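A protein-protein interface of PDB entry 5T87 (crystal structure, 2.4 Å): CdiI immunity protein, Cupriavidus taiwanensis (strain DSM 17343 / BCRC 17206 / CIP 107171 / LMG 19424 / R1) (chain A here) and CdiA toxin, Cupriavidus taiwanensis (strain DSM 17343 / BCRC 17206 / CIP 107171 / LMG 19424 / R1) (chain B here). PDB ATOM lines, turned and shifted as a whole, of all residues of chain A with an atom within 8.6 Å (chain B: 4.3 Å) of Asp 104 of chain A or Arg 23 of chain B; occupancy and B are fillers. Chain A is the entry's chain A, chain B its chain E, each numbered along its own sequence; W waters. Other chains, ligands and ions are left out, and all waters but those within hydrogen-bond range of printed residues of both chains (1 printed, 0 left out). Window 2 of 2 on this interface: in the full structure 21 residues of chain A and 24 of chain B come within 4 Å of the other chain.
OD1 of Asp 108 of chain A is in salt-bridge range of NH2 of Arg 50 of chain B (2.7 Å). NH1 of Arg 23 of chain B sits at hydrogen-bond distance from O of Asp 104 of chain A, at 3.3 Å. The side-chain carboxylate (OD2) of Asp 104 of chain A lies within hydrogen-bond range of the side-chain hydroxyl (OG) of Ser 21 of chain B (2.6 Å). The side-chain carboxylate (OD1) of Asp 108 of chain A lies within salt-bridge range of the guanidinium group (NH1) of Arg 23 of chain B.
The guanidinium group of Arg 75 of chain A is in hydrogen-bond range of a ring nitrogen (ND1) of His 72 of chain A (3.2 Å). The backbone NH of Val 17 of chain B lies within hydrogen-bond range of the backbone carbonyl oxygen of Arg 23 of chain B (3.0 Å). NE2 of Gln 16 of chain B is in hydrogen-bond range of O of Ser 21 of chain B, at 2.8 Å. The backbone NH (N) of Arg 23 of chain B lies within hydrogen-bond range of the side-chain hydroxyl (OG) of Ser 21 of chain B (3.0 Å). The side-chain carboxylate of Asp 38 of chain B is in salt-bridge range of the guanidinium group of Arg 23 of chain B (2.7 Å).
Among the printed residues, pairs that only touch across the chains: His 72 of chain A with Asp 38 of chain B (3.4 Å), Ser 100 of chain A with Ser 21 of chain B (3.5 Å) and Phe 112 of chain A with Arg 50 of chain B (3.7 Å).
Of the printed residues of chain B, His 72 of chain A touches Asp 38 (3.4 Å). Printed residues of chain A within 4 Å of Ser 21 of chain B: Ser 100 (3.5 Å) and Asp 104 (2.6 Å). Arg 23 of chain B touches just these residues of chain A: Asp 104 and Asp 108. Printed residues of chain A within 4 Å of Asp 38 of chain B: His 72. Of the printed residues of chain A, Arg 50 of chain B touches Asp 108 and Phe 112. The nearest residue of chain A that does not touch Arg 23 of chain B is His 72 of chain A (4.4 Å).
Along chain B the printed residues that touch a printed residue of chain A span positions 21 to 50. Of the 26 printed residues of chain A, 5 touch a printed residue of chain B. Among the printed residues, Asp or Glu carboxylates within 4 Å of a Lys or Arg side-chain nitrogen of the other chain: Asp 108 of chain A with Arg 23 of chain B (2.8 Å) and Asp 108 of chain A with Arg 50 of chain B (2.7 Å).
Water W1 lies within hydrogen-bond range of the side-chain carboxylate of Asp 108 of chain A (2.9 Å), the backbone carbonyl oxygen of Thr 68 of chain A (3.1 Å) and the guanidinium group of Arg 23 of chain B (3.3 Å).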
ATOM      1  N   TYR A  37      19.848 -14.992  -5.447  1.00  0.00           N
ATOM      2  CA  TYR A  37      20.642 -14.681  -4.249  1.00  0.00           C
ATOM      3  C   TYR A  37      21.406 -15.859  -3.666  1.00  0.00           C
ATOM      4  O   TYR A  37      22.449 -15.649  -3.050  1.00  0.00           O
ATOM      5  CB  TYR A  37      19.754 -14.065  -3.122  1.00  0.00           C
ATOM      6  CG  TYR A  37      19.550 -12.560  -3.186  1.00  0.00           C
ATOM      7  CD1 TYR A  37      19.363 -11.924  -4.408  1.00  0.00           C
ATOM      8  CD2 TYR A  37      19.497 -11.776  -2.015  1.00  0.00           C
ATOM      9  CE1 TYR A  37      19.162 -10.556  -4.482  1.00  0.00           C
ATOM     10  CE2 TYR A  37      19.274 -10.395  -2.079  1.00  0.00           C
ATOM     11  CZ  TYR A  37      19.114  -9.791  -3.328  1.00  0.00           C
ATOM     12  OH  TYR A  37      18.924  -8.439  -3.510  1.00  0.00           O
ATOM     13  N   SER A  64      10.422  -9.499 -16.507  1.00  0.00           N
ATOM     14  CA  SER A  64      11.375  -8.447 -16.207  1.00  0.00           C
ATOM     15  C   SER A  64      12.200  -8.762 -14.954  1.00  0.00           C
ATOM     16  O   SER A  64      13.425  -8.559 -14.937  1.00  0.00           O
ATOM     17  CB  SER A  64      10.631  -7.114 -16.055  1.00  0.00           C
ATOM     18  OG  SER A  64      11.526  -6.021 -16.148  1.00  0.00           O
ATOM     19  N   VAL A  67      14.941 -11.351 -15.642  1.00  0.00           N
ATOM     20  CA  VAL A  67      16.112 -10.715 -16.248  1.00  0.00           C
ATOM     21  C   VAL A  67      16.974 -10.042 -15.188  1.00  0.00           C
ATOM     22  O   VAL A  67      18.155 -10.252 -15.137  1.00  0.00           O
ATOM     23  CB  VAL A  67      15.698  -9.684 -17.302  1.00  0.00           C
ATOM     24  CG1 VAL A  67      16.885  -8.833 -17.751  1.00  0.00           C
ATOM     25  CG2 VAL A  67      15.073 -10.386 -18.495  1.00  0.00           C
ATOM     26  N   THR A  68      16.356  -9.235 -14.335  1.00  0.00           N
ATOM     27  CA  THR A  68      17.052  -8.608 -13.217  1.00  0.00           C
ATOM     28  C   THR A  68      17.776  -9.663 -12.374  1.00  0.00           C
ATOM     29  O   THR A  68      18.927  -9.469 -11.992  1.00  0.00           O
ATOM     30  CB  THR A  68      16.064  -7.746 -12.384  1.00  0.00           C
ATOM     31  OG1 THR A  68      15.809  -6.531 -13.095  1.00  0.00           O
ATOM     32  CG2 THR A  68      16.601  -7.394 -10.998  1.00  0.00           C
ATOM     33  N   CYS A  69      17.109 -10.783 -12.124  1.00  0.00           N
ATOM     34  CA  CYS A  69      17.732 -11.915 -11.437  1.00  0.00           C
ATOM     35  C   CYS A  69      18.949 -12.491 -12.167  1.00  0.00           C
ATOM     36  O   CYS A  69      19.918 -12.906 -11.525  1.00  0.00           O
ATOM     37  CB  CYS A  69      16.711 -13.021 -11.188  1.00  0.00           C
ATOM     38  SG  CYS A  69      15.608 -12.613  -9.832  1.00  0.00           S
ATOM     39  N   VAL A  70      18.908 -12.505 -13.497  1.00  0.00           N
ATOM     40  CA  VAL A  70      20.086 -12.929 -14.283  1.00  0.00           C
ATOM     41  C   VAL A  70      21.243 -11.960 -14.015  1.00  0.00           C
ATOM     42  O   VAL A  70      22.407 -12.382 -13.906  1.00  0.00           O
ATOM     43  CB  VAL A  70      19.762 -13.082 -15.797  1.00  0.00           C
ATOM     44  CG1 VAL A  70      21.021 -13.249 -16.648  1.00  0.00           C
ATOM     45  CG2 VAL A  70      18.832 -14.272 -16.018  1.00  0.00           C
ATOM     46  N   GLY A  71      20.901 -10.677 -13.869  1.00  0.00           N
ATOM     47  CA  GLY A  71      21.845  -9.647 -13.441  1.00  0.00           C
ATOM     48  C   GLY A  71      22.484  -9.946 -12.107  1.00  0.00           C
ATOM     49  O   GLY A  71      23.676  -9.715 -11.923  1.00  0.00           O
ATOM     50  N   HIS A  72      21.687 -10.468 -11.182  1.00  0.00           N
ATOM     51  CA  HIS A  72      22.181 -10.817  -9.856  1.00  0.00           C
ATOM     52  C   HIS A  72      23.116 -11.995  -9.904  1.00  0.00           C
ATOM     53  O   HIS A  72      24.168 -11.965  -9.257  1.00  0.00           O
ATOM     54  CB  HIS A  72      21.037 -11.115  -8.886  1.00  0.00           C
ATOM     55  CG  HIS A  72      20.175  -9.936  -8.610  1.00  0.00           C
ATOM     56  ND1 HIS A  72      20.686  -8.669  -8.436  1.00  0.00           N
ATOM     57  CD2 HIS A  72      18.834  -9.822  -8.484  1.00  0.00           C
ATOM     58  CE1 HIS A  72      19.698  -7.823  -8.208  1.00  0.00           C
ATOM     59  NE2 HIS A  72      18.564  -8.497  -8.239  1.00  0.00           N
ATOM     60  N   ALA A  74      24.980 -12.914 -12.395  1.00  0.00           N
ATOM     61  CA  ALA A  74      26.198 -12.406 -13.025  1.00  0.00           C
ATOM     62  C   ALA A  74      27.103 -11.675 -12.033  1.00  0.00           C
ATOM     63  O   ALA A  74      28.321 -11.859 -12.038  1.00  0.00           O
ATOM     64  CB  ALA A  74      25.844 -11.475 -14.172  1.00  0.00           C
ATOM     65  N   ARG A  75      26.488 -10.839 -11.208  1.00  0.00           N
ATOM     66  CA  ARG A  75      27.175 -10.163 -10.121  1.00  0.00           C
ATOM     67  C   ARG A  75      27.883 -11.140  -9.164  1.00  0.00           C
ATOM     68  O   ARG A  75      29.003 -10.875  -8.726  1.00  0.00           O
ATOM     69  CB  ARG A  75      26.180  -9.266  -9.353  1.00  0.00           C
ATOM     70  CG  ARG A  75      26.680  -8.751  -8.014  1.00  0.00           C
ATOM     71  CD  ARG A  75      25.819  -7.619  -7.478  1.00  0.00           C
ATOM     72  NE  ARG A  75      24.430  -7.987  -7.160  1.00  0.00           N
ATOM     73  CZ  ARG A  75      24.034  -8.732  -6.123  1.00  0.00           C
ATOM     74  NH1 ARG A  75      24.917  -9.262  -5.276  1.00  0.00           N
ATOM     75  NH2 ARG A  75      22.739  -8.969  -5.939  1.00  0.00           N
ATOM     76  N   LEU A  89      21.179 -11.231 -22.795  1.00  0.00           N
ATOM     77  CA  LEU A  89      20.734  -9.894 -22.426  1.00  0.00           C
ATOM     78  C   LEU A  89      20.609  -8.970 -23.636  1.00  0.00           C
ATOM     79  O   LEU A  89      19.678  -8.150 -23.700  1.00  0.00           O
ATOM     80  CB  LEU A  89      21.668  -9.290 -21.383  1.00  0.00           C
ATOM     81  CG  LEU A  89      21.718 -10.027 -20.040  1.00  0.00           C
ATOM     82  CD1 LEU A  89      22.836  -9.474 -19.168  1.00  0.00           C
ATOM     83  CD2 LEU A  89      20.385  -9.951 -19.318  1.00  0.00           C
ATOM     84  N   VAL A  98      10.838  -6.263 -21.207  1.00  0.00           N
ATOM     85  CA  VAL A  98      12.059  -6.569 -20.447  1.00  0.00           C
ATOM     86  C   VAL A  98      13.262  -5.665 -20.700  1.00  0.00           C
ATOM     87  O   VAL A  98      14.228  -5.727 -19.937  1.00  0.00           O
ATOM     88  CB  VAL A  98      12.443  -8.045 -20.616  1.00  0.00           C
ATOM     89  CG1 VAL A  98      11.360  -8.925 -20.005  1.00  0.00           C
ATOM     90  CG2 VAL A  98      12.662  -8.412 -22.084  1.00  0.00           C
ATOM     91  N   ALA A  99      13.186  -4.807 -21.717  1.00  0.00           N
ATOM     92  CA  ALA A  99      14.325  -3.970 -22.126  1.00  0.00           C
ATOM     93  C   ALA A  99      15.014  -3.274 -20.961  1.00  0.00           C
ATOM     94  O   ALA A  99      16.226  -3.352 -20.810  1.00  0.00           O
ATOM     95  CB  ALA A  99      13.892  -2.938 -23.158  1.00  0.00           C
ATOM     96  N   SER A 100      14.233  -2.615 -20.134  1.00  0.00           N
ATOM     97  CA  SER A 100      14.779  -1.807 -19.056  1.00  0.00           C
ATOM     98  C   SER A 100      15.636  -2.631 -18.054  1.00  0.00           C
ATOM     99  O   SER A 100      16.751  -2.231 -17.684  1.00  0.00           O
ATOM    100  CB  SER A 100      13.632  -1.061 -18.368  1.00  0.00           C
ATOM    101  OG  SER A 100      13.997  -0.673 -17.067  1.00  0.00           O
ATOM    102  N   ALA A 101      15.109  -3.774 -17.629  1.00  0.00           N
ATOM    103  CA  ALA A 101      15.836  -4.694 -16.757  1.00  0.00           C
ATOM    104  C   ALA A 101      17.039  -5.334 -17.471  1.00  0.00           C
ATOM    105  O   ALA A 101      18.051  -5.637 -16.829  1.00  0.00           O
ATOM    106  CB  ALA A 101      14.907  -5.788 -16.251  1.00  0.00           C
ATOM    107  N   ALA A 102      16.908  -5.576 -18.781  1.00  0.00           N
ATOM    108  CA  ALA A 102      18.029  -6.073 -19.601  1.00  0.00           C
ATOM    109  C   ALA A 102      19.211  -5.119 -19.537  1.00  0.00           C
ATOM    110  O   ALA A 102      20.327  -5.543 -19.275  1.00  0.00           O
ATOM    111  CB  ALA A 102      17.605  -6.291 -21.051  1.00  0.00           C
ATOM    112  N   SER A 103      18.945  -3.833 -19.741  1.00  0.00           N
ATOM    113  CA  SER A 103      19.958  -2.788 -19.627  1.00  0.00           C
ATOM    114  C   SER A 103      20.671  -2.793 -18.267  1.00  0.00           C
ATOM    115  O   SER A 103      21.887  -2.703 -18.216  1.00  0.00           O
ATOM    116  CB  SER A 103      19.318  -1.421 -19.874  1.00  0.00           C
ATOM    117  OG  SER A 103      20.289  -0.396 -19.853  1.00  0.00           O
ATOM    118  N   ASP A 104      19.919  -2.905 -17.177  1.00  0.00           N
ATOM    119  CA  ASP A 104      20.497  -2.913 -15.825  1.00  0.00           C
ATOM    120  C   ASP A 104      21.192  -4.237 -15.490  1.00  0.00           C
ATOM    121  O   ASP A 104      22.113  -4.271 -14.671  1.00  0.00           O
ATOM    122  CB  ASP A 104      19.428  -2.648 -14.763  1.00  0.00           C
ATOM    123  CG  ASP A 104      18.777  -1.274 -14.889  1.00  0.00           C
ATOM    124  OD1 ASP A 104      19.310  -0.381 -15.593  1.00  0.00           O
ATOM    125  OD2 ASP A 104      17.716  -1.088 -14.256  1.00  0.00           O
ATOM    126  N   ALA A 105      20.728  -5.335 -16.084  1.00  0.00           N
ATOM    127  CA  ALA A 105      21.389  -6.624 -15.912  1.00  0.00           C
ATOM    128  C   ALA A 105      22.754  -6.602 -16.624  1.00  0.00           C
ATOM    129  O   ALA A 105      23.749  -7.134 -16.125  1.00  0.00           O
ATOM    130  CB  ALA A 105      20.510  -7.738 -16.446  1.00  0.00           C
ATOM    131  N   LEU A 106      22.772  -5.952 -17.782  1.00  0.00           N
ATOM    132  CA  LEU A 106      23.979  -5.733 -18.565  1.00  0.00           C
ATOM    133  C   LEU A 106      25.003  -4.851 -17.822  1.00  0.00           C
ATOM    134  O   LEU A 106      26.204  -5.142 -17.832  1.00  0.00           O
ATOM    135  CB  LEU A 106      23.590  -5.090 -19.896  1.00  0.00           C
ATOM    136  CG  LEU A 106      24.424  -5.380 -21.128  1.00  0.00           C
ATOM    137  CD1 LEU A 106      24.506  -6.884 -21.389  1.00  0.00           C
ATOM    138  CD2 LEU A 106      23.789  -4.644 -22.311  1.00  0.00           C
ATOM    139  N   ASP A 107      24.515  -3.783 -17.180  1.00  0.00           N
ATOM    140  CA  ASP A 107      25.320  -3.001 -16.230  1.00  0.00           C
ATOM    141  C   ASP A 107      25.974  -3.932 -15.209  1.00  0.00           C
ATOM    142  O   ASP A 107      27.160  -3.806 -14.942  1.00  0.00           O
ATOM    143  CB  ASP A 107      24.468  -1.945 -15.488  1.00  0.00           C
ATOM    144  CG  ASP A 107      24.172  -0.698 -16.335  1.00  0.00           C
ATOM    145  OD1 ASP A 107      24.563  -0.663 -17.523  1.00  0.00           O
ATOM    146  OD2 ASP A 107      23.546   0.259 -15.801  1.00  0.00           O
ATOM    147  N   ASP A 108      25.195  -4.869 -14.663  1.00  0.00           N
ATOM    148  CA  ASP A 108      25.696  -5.822 -13.669  1.00  0.00           C
ATOM    149  C   ASP A 108      26.772  -6.731 -14.260  1.00  0.00           C
ATOM    150  O   ASP A 108      27.806  -6.964 -13.628  1.00  0.00           O
ATOM    151  CB  ASP A 108      24.542  -6.645 -13.043  1.00  0.00           C
ATOM    152  CG  ASP A 108      23.567  -5.782 -12.216  1.00  0.00           C
ATOM    153  OD1 ASP A 108      23.779  -4.546 -12.120  1.00  0.00           O
ATOM    154  OD2 ASP A 108      22.595  -6.340 -11.651  1.00  0.00           O
ATOM    155  N   LEU A 109      26.541  -7.208 -15.481  1.00  0.00           N
ATOM    156  CA  LEU A 109      27.503  -8.065 -16.175  1.00  0.00           C
ATOM    157  C   LEU A 109      28.826  -7.346 -16.429  1.00  0.00           C
ATOM    158  O   LEU A 109      29.891  -7.842 -16.051  1.00  0.00           O
ATOM    159  CB  LEU A 109      26.932  -8.557 -17.507  1.00  0.00           C
ATOM    160  CG  LEU A 109      27.699  -9.682 -18.211  1.00  0.00           C
ATOM    161  CD1 LEU A 109      27.765 -10.928 -17.338  1.00  0.00           C
ATOM    162  CD2 LEU A 109      27.078 -10.012 -19.565  1.00  0.00           C
ATOM    163  N   ARG A 110      28.735  -6.164 -17.029  1.00  0.00           N
ATOM    164  CA  ARG A 110      29.912  -5.390 -17.425  1.00  0.00           C
ATOM    165  C   ARG A 110      30.794  -4.976 -16.227  1.00  0.00           C
ATOM    166  O   ARG A 110      32.021  -4.925 -16.341  1.00  0.00           O
ATOM    167  CB  ARG A 110      29.493  -4.147 -18.225  1.00  0.00           C
ATOM    168  CG  ARG A 110      28.696  -4.424 -19.508  1.00  0.00           C
ATOM    169  CD  ARG A 110      29.582  -4.741 -20.704  1.00  0.00           C
ATOM    170  NE  ARG A 110      28.883  -5.384 -21.835  1.00  0.00           N
ATOM    171  CZ  ARG A 110      28.077  -4.772 -22.715  1.00  0.00           C
ATOM    172  NH1 ARG A 110      27.531  -5.479 -23.712  1.00  0.00           N
ATOM    173  NH2 ARG A 110      27.795  -3.465 -22.606  1.00  0.00           N
ATOM    174  N   ILE A 111      30.169  -4.693 -15.088  1.00  0.00           N
ATOM    175  CA  ILE A 111      30.885  -4.239 -13.898  1.00  0.00           C
ATOM    176  C   ILE A 111      31.584  -5.423 -13.229  1.00  0.00           C
ATOM    177  O   ILE A 111      32.808  -5.427 -13.064  1.00  0.00           O
ATOM    178  CB  ILE A 111      29.923  -3.559 -12.885  1.00  0.00           C
ATOM    179  CG1 ILE A 111      29.437  -2.191 -13.408  1.00  0.00           C
ATOM    180  CG2 ILE A 111      30.560  -3.435 -11.503  1.00  0.00           C
ATOM    181  CD1 ILE A 111      30.399  -1.033 -13.209  1.00  0.00           C
ATOM    182  N   PHE A 112      30.793  -6.413 -12.836  1.00  0.00           N
ATOM    183  CA  PHE A 112      31.286  -7.504 -12.005  1.00  0.00           C
ATOM    184  C   PHE A 112      32.083  -8.547 -12.761  1.00  0.00           C
ATOM    185  O   PHE A 112      32.834  -9.293 -12.143  1.00  0.00           O
ATOM    186  CB  PHE A 112      30.126  -8.167 -11.243  1.00  0.00           C
ATOM    187  CG  PHE A 112      29.626  -7.336 -10.113  1.00  0.00           C
ATOM    188  CD1 PHE A 112      30.255  -7.383  -8.879  1.00  0.00           C
ATOM    189  CD2 PHE A 112      28.563  -6.466 -10.291  1.00  0.00           C
ATOM    190  CE1 PHE A 112      29.823  -6.586  -7.829  1.00  0.00           C
ATOM    191  CE2 PHE A 112      28.125  -5.665  -9.247  1.00  0.00           C
ATOM    192  CZ  PHE A 112      28.758  -5.722  -8.013  1.00  0.00           C
ATOM    193  N   GLN B  16      15.598   7.056  -7.314  1.00  0.00           N
ATOM    194  CA  GLN B  16      15.560   6.355  -8.586  1.00  0.00           C
ATOM    195  C   GLN B  16      16.726   6.845  -9.414  1.00  0.00           C
ATOM    196  O   GLN B  16      16.988   8.037  -9.448  1.00  0.00           O
ATOM    197  CB  GLN B  16      14.246   6.652  -9.306  1.00  0.00           C
ATOM    198  CG  GLN B  16      14.062   5.901 -10.612  1.00  0.00           C
ATOM    199  CD  GLN B  16      12.657   6.015 -11.168  1.00  0.00           C
ATOM    200  OE1 GLN B  16      11.802   6.676 -10.591  1.00  0.00           O
ATOM    201  NE2 GLN B  16      12.415   5.369 -12.296  1.00  0.00           N
ATOM    202  N   VAL B  17      17.419   5.931 -10.079  1.00  0.00           N
ATOM    203  CA  VAL B  17      18.627   6.279 -10.824  1.00  0.00           C
ATOM    204  C   VAL B  17      18.250   6.934 -12.154  1.00  0.00           C
ATOM    205  O   VAL B  17      18.840   7.945 -12.543  1.00  0.00           O
ATOM    206  CB  VAL B  17      19.538   5.047 -11.074  1.00  0.00           C
ATOM    207  CG1 VAL B  17      20.822   5.457 -11.794  1.00  0.00           C
ATOM    208  CG2 VAL B  17      19.881   4.351  -9.761  1.00  0.00           C
ATOM    209  N   LYS B  18      17.282   6.335 -12.847  1.00  0.00           N
ATOM    210  CA  LYS B  18      16.800   6.820 -14.139  1.00  0.00           C
ATOM    211  C   LYS B  18      15.308   6.588 -14.200  1.00  0.00           C
ATOM    212  O   LYS B  18      14.840   5.549 -13.743  1.00  0.00           O
ATOM    213  CB  LYS B  18      17.446   6.031 -15.271  1.00  0.00           C
ATOM    214  CG  LYS B  18      18.913   5.720 -15.062  1.00  0.00           C
ATOM    215  CD  LYS B  18      19.537   5.102 -16.299  1.00  0.00           C
ATOM    216  CE  LYS B  18      19.054   3.680 -16.521  1.00  0.00           C
ATOM    217  NZ  LYS B  18      19.857   3.043 -17.590  1.00  0.00           N
ATOM    218  N   SER B  21      13.888   3.202 -15.496  1.00  0.00           N
ATOM    219  CA  SER B  21      14.052   1.992 -14.695  1.00  0.00           C
ATOM    220  C   SER B  21      13.686   2.211 -13.241  1.00  0.00           C
ATOM    221  O   SER B  21      14.108   3.197 -12.654  1.00  0.00           O
ATOM    222  CB  SER B  21      15.507   1.517 -14.739  1.00  0.00           C
ATOM    223  OG  SER B  21      15.760   0.550 -13.730  1.00  0.00           O
ATOM    224  N   PRO B  22      12.982   1.241 -12.627  1.00  0.00           N
ATOM    225  CA  PRO B  22      12.699   1.328 -11.193  1.00  0.00           C
ATOM    226  C   PRO B  22      13.918   1.147 -10.278  1.00  0.00           C
ATOM    227  O   PRO B  22      13.790   1.315  -9.078  1.00  0.00           O
ATOM    228  CB  PRO B  22      11.713   0.179 -10.972  1.00  0.00           C
ATOM    229  CG  PRO B  22      12.096  -0.838 -11.996  1.00  0.00           C
ATOM    230  CD  PRO B  22      12.565  -0.060 -13.189  1.00  0.00           C
ATOM    231  N   ARG B  23      15.078   0.788 -10.828  1.00  0.00           N
ATOM    232  CA  ARG B  23      16.296   0.661 -10.031  1.00  0.00           C
ATOM    233  C   ARG B  23      16.611   1.944  -9.266  1.00  0.00           C
ATOM    234  O   ARG B  23      16.693   3.019  -9.865  1.00  0.00           O
ATOM    235  CB  ARG B  23      17.481   0.295 -10.917  1.00  0.00           C
ATOM    236  CG  ARG B  23      18.783   0.075 -10.161  1.00  0.00           C
ATOM    237  CD  ARG B  23      19.783  -0.730 -10.981  1.00  0.00           C
ATOM    238  NE  ARG B  23      19.776  -2.152 -10.640  1.00  0.00           N
ATOM    239  CZ  ARG B  23      20.685  -3.044 -11.046  1.00  0.00           C
ATOM    240  NH1 ARG B  23      21.692  -2.677 -11.838  1.00  0.00           N
ATOM    241  NH2 ARG B  23      20.580  -4.313 -10.658  1.00  0.00           N
ATOM    242  N   ARG B  24      16.772   1.796  -7.947  1.00  0.00           N
ATOM    243  CA  ARG B  24      17.092   2.885  -7.045  1.00  0.00           C
ATOM    244  C   ARG B  24      18.446   2.656  -6.393  1.00  0.00           C
ATOM    245  O   ARG B  24      19.008   1.552  -6.461  1.00  0.00           O
ATOM    246  CB  ARG B  24      16.048   2.994  -5.931  1.00  0.00           C
ATOM    247  CG  ARG B  24      14.603   2.954  -6.389  1.00  0.00           C
ATOM    248  CD  ARG B  24      13.660   3.230  -5.229  1.00  0.00           C
ATOM    249  NE  ARG B  24      13.674   4.636  -4.808  1.00  0.00           N
ATOM    250  CZ  ARG B  24      13.037   5.642  -5.421  1.00  0.00           C
ATOM    251  NH1 ARG B  24      13.131   6.873  -4.931  1.00  0.00           N
ATOM    252  NH2 ARG B  24      12.315   5.439  -6.519  1.00  0.00           N
ATOM    253  N   VAL B  36      22.007  -0.932  -3.609  1.00  0.00           N
ATOM    254  CA  VAL B  36      21.213  -0.961  -4.844  1.00  0.00           C
ATOM    255  C   VAL B  36      19.919  -1.738  -4.595  1.00  0.00           C
ATOM    256  O   VAL B  36      19.950  -2.864  -4.071  1.00  0.00           O
ATOM    257  CB  VAL B  36      21.979  -1.647  -5.990  1.00  0.00           C
ATOM    258  CG1 VAL B  36      21.112  -1.750  -7.249  1.00  0.00           C
ATOM    259  CG2 VAL B  36      23.286  -0.924  -6.292  1.00  0.00           C
ATOM    260  N   PHE B  37      18.797  -1.134  -4.997  1.00  0.00           N
ATOM    261  CA  PHE B  37      17.463  -1.697  -4.805  1.00  0.00           C
ATOM    262  C   PHE B  37      16.777  -1.926  -6.128  1.00  0.00           C
ATOM    263  O   PHE B  37      16.810  -1.057  -6.989  1.00  0.00           O
ATOM    264  CB  PHE B  37      16.600  -0.717  -4.026  1.00  0.00           C
ATOM    265  CG  PHE B  37      17.028  -0.529  -2.608  1.00  0.00           C
ATOM    266  CD1 PHE B  37      16.763  -1.513  -1.659  1.00  0.00           C
ATOM    267  CD2 PHE B  37      17.675   0.639  -2.207  1.00  0.00           C
ATOM    268  CE1 PHE B  37      17.152  -1.350  -0.336  1.00  0.00           C
ATOM    269  CE2 PHE B  37      18.056   0.814  -0.881  1.00  0.00           C
ATOM    270  CZ  PHE B  37      17.793  -0.186   0.054  1.00  0.00           C
ATOM    271  N   ASP B  38      16.108  -3.065  -6.257  1.00  0.00           N
ATOM    272  CA  ASP B  38      15.368  -3.406  -7.472  1.00  0.00           C
ATOM    273  C   ASP B  38      13.961  -3.833  -7.122  1.00  0.00           C
ATOM    274  O   ASP B  38      13.723  -4.384  -6.048  1.00  0.00           O
ATOM    275  CB  ASP B  38      16.057  -4.553  -8.202  1.00  0.00           C
ATOM    276  CG  ASP B  38      17.472  -4.219  -8.593  1.00  0.00           C
ATOM    277  OD1 ASP B  38      17.634  -3.456  -9.571  1.00  0.00           O
ATOM    278  OD2 ASP B  38      18.412  -4.697  -7.907  1.00  0.00           O
ATOM    279  N   ARG B  50      26.988  -2.695  -2.380  1.00  0.00           N
ATOM    280  CA  ARG B  50      28.060  -2.522  -3.358  1.00  0.00           C
ATOM    281  C   ARG B  50      29.206  -1.638  -2.852  1.00  0.00           C
ATOM    282  O   ARG B  50      29.021  -0.814  -1.964  1.00  0.00           O
ATOM    283  CB  ARG B  50      27.504  -1.963  -4.672  1.00  0.00           C
ATOM    284  CG  ARG B  50      26.800  -2.987  -5.551  1.00  0.00           C
ATOM    285  CD  ARG B  50      26.706  -2.500  -6.992  1.00  0.00           C
ATOM    286  NE  ARG B  50      25.743  -3.280  -7.773  1.00  0.00           N
ATOM    287  CZ  ARG B  50      25.443  -3.064  -9.057  1.00  0.00           C
ATOM    288  NH1 ARG B  50      26.073  -2.124  -9.760  1.00  0.00           N
ATOM    289  NH2 ARG B  50      24.542  -3.834  -9.656  1.00  0.00           N
ATOM    290  N   MET B  59      24.714   6.111 -11.197  1.00  0.00           N
ATOM    291  CA  MET B  59      24.463   5.796  -9.777  1.00  0.00           C
ATOM    292  C   MET B  59      25.173   6.762  -8.873  1.00  0.00           C
ATOM    293  O   MET B  59      24.582   7.298  -7.930  1.00  0.00           O
ATOM    294  CB  MET B  59      24.930   4.376  -9.418  1.00  0.00           C
ATOM    295  CG  MET B  59      24.139   3.269 -10.134  1.00  0.00           C
ATOM    296  SD  MET B  59      24.366   1.475  -9.306  1.00  0.00           S
ATOM    297  CE  MET B  59      23.866   0.338 -10.841  1.00  0.00           C
HETATM  298  O   HOH W   1      19.970  -6.720 -12.860  1.00  0.00           O
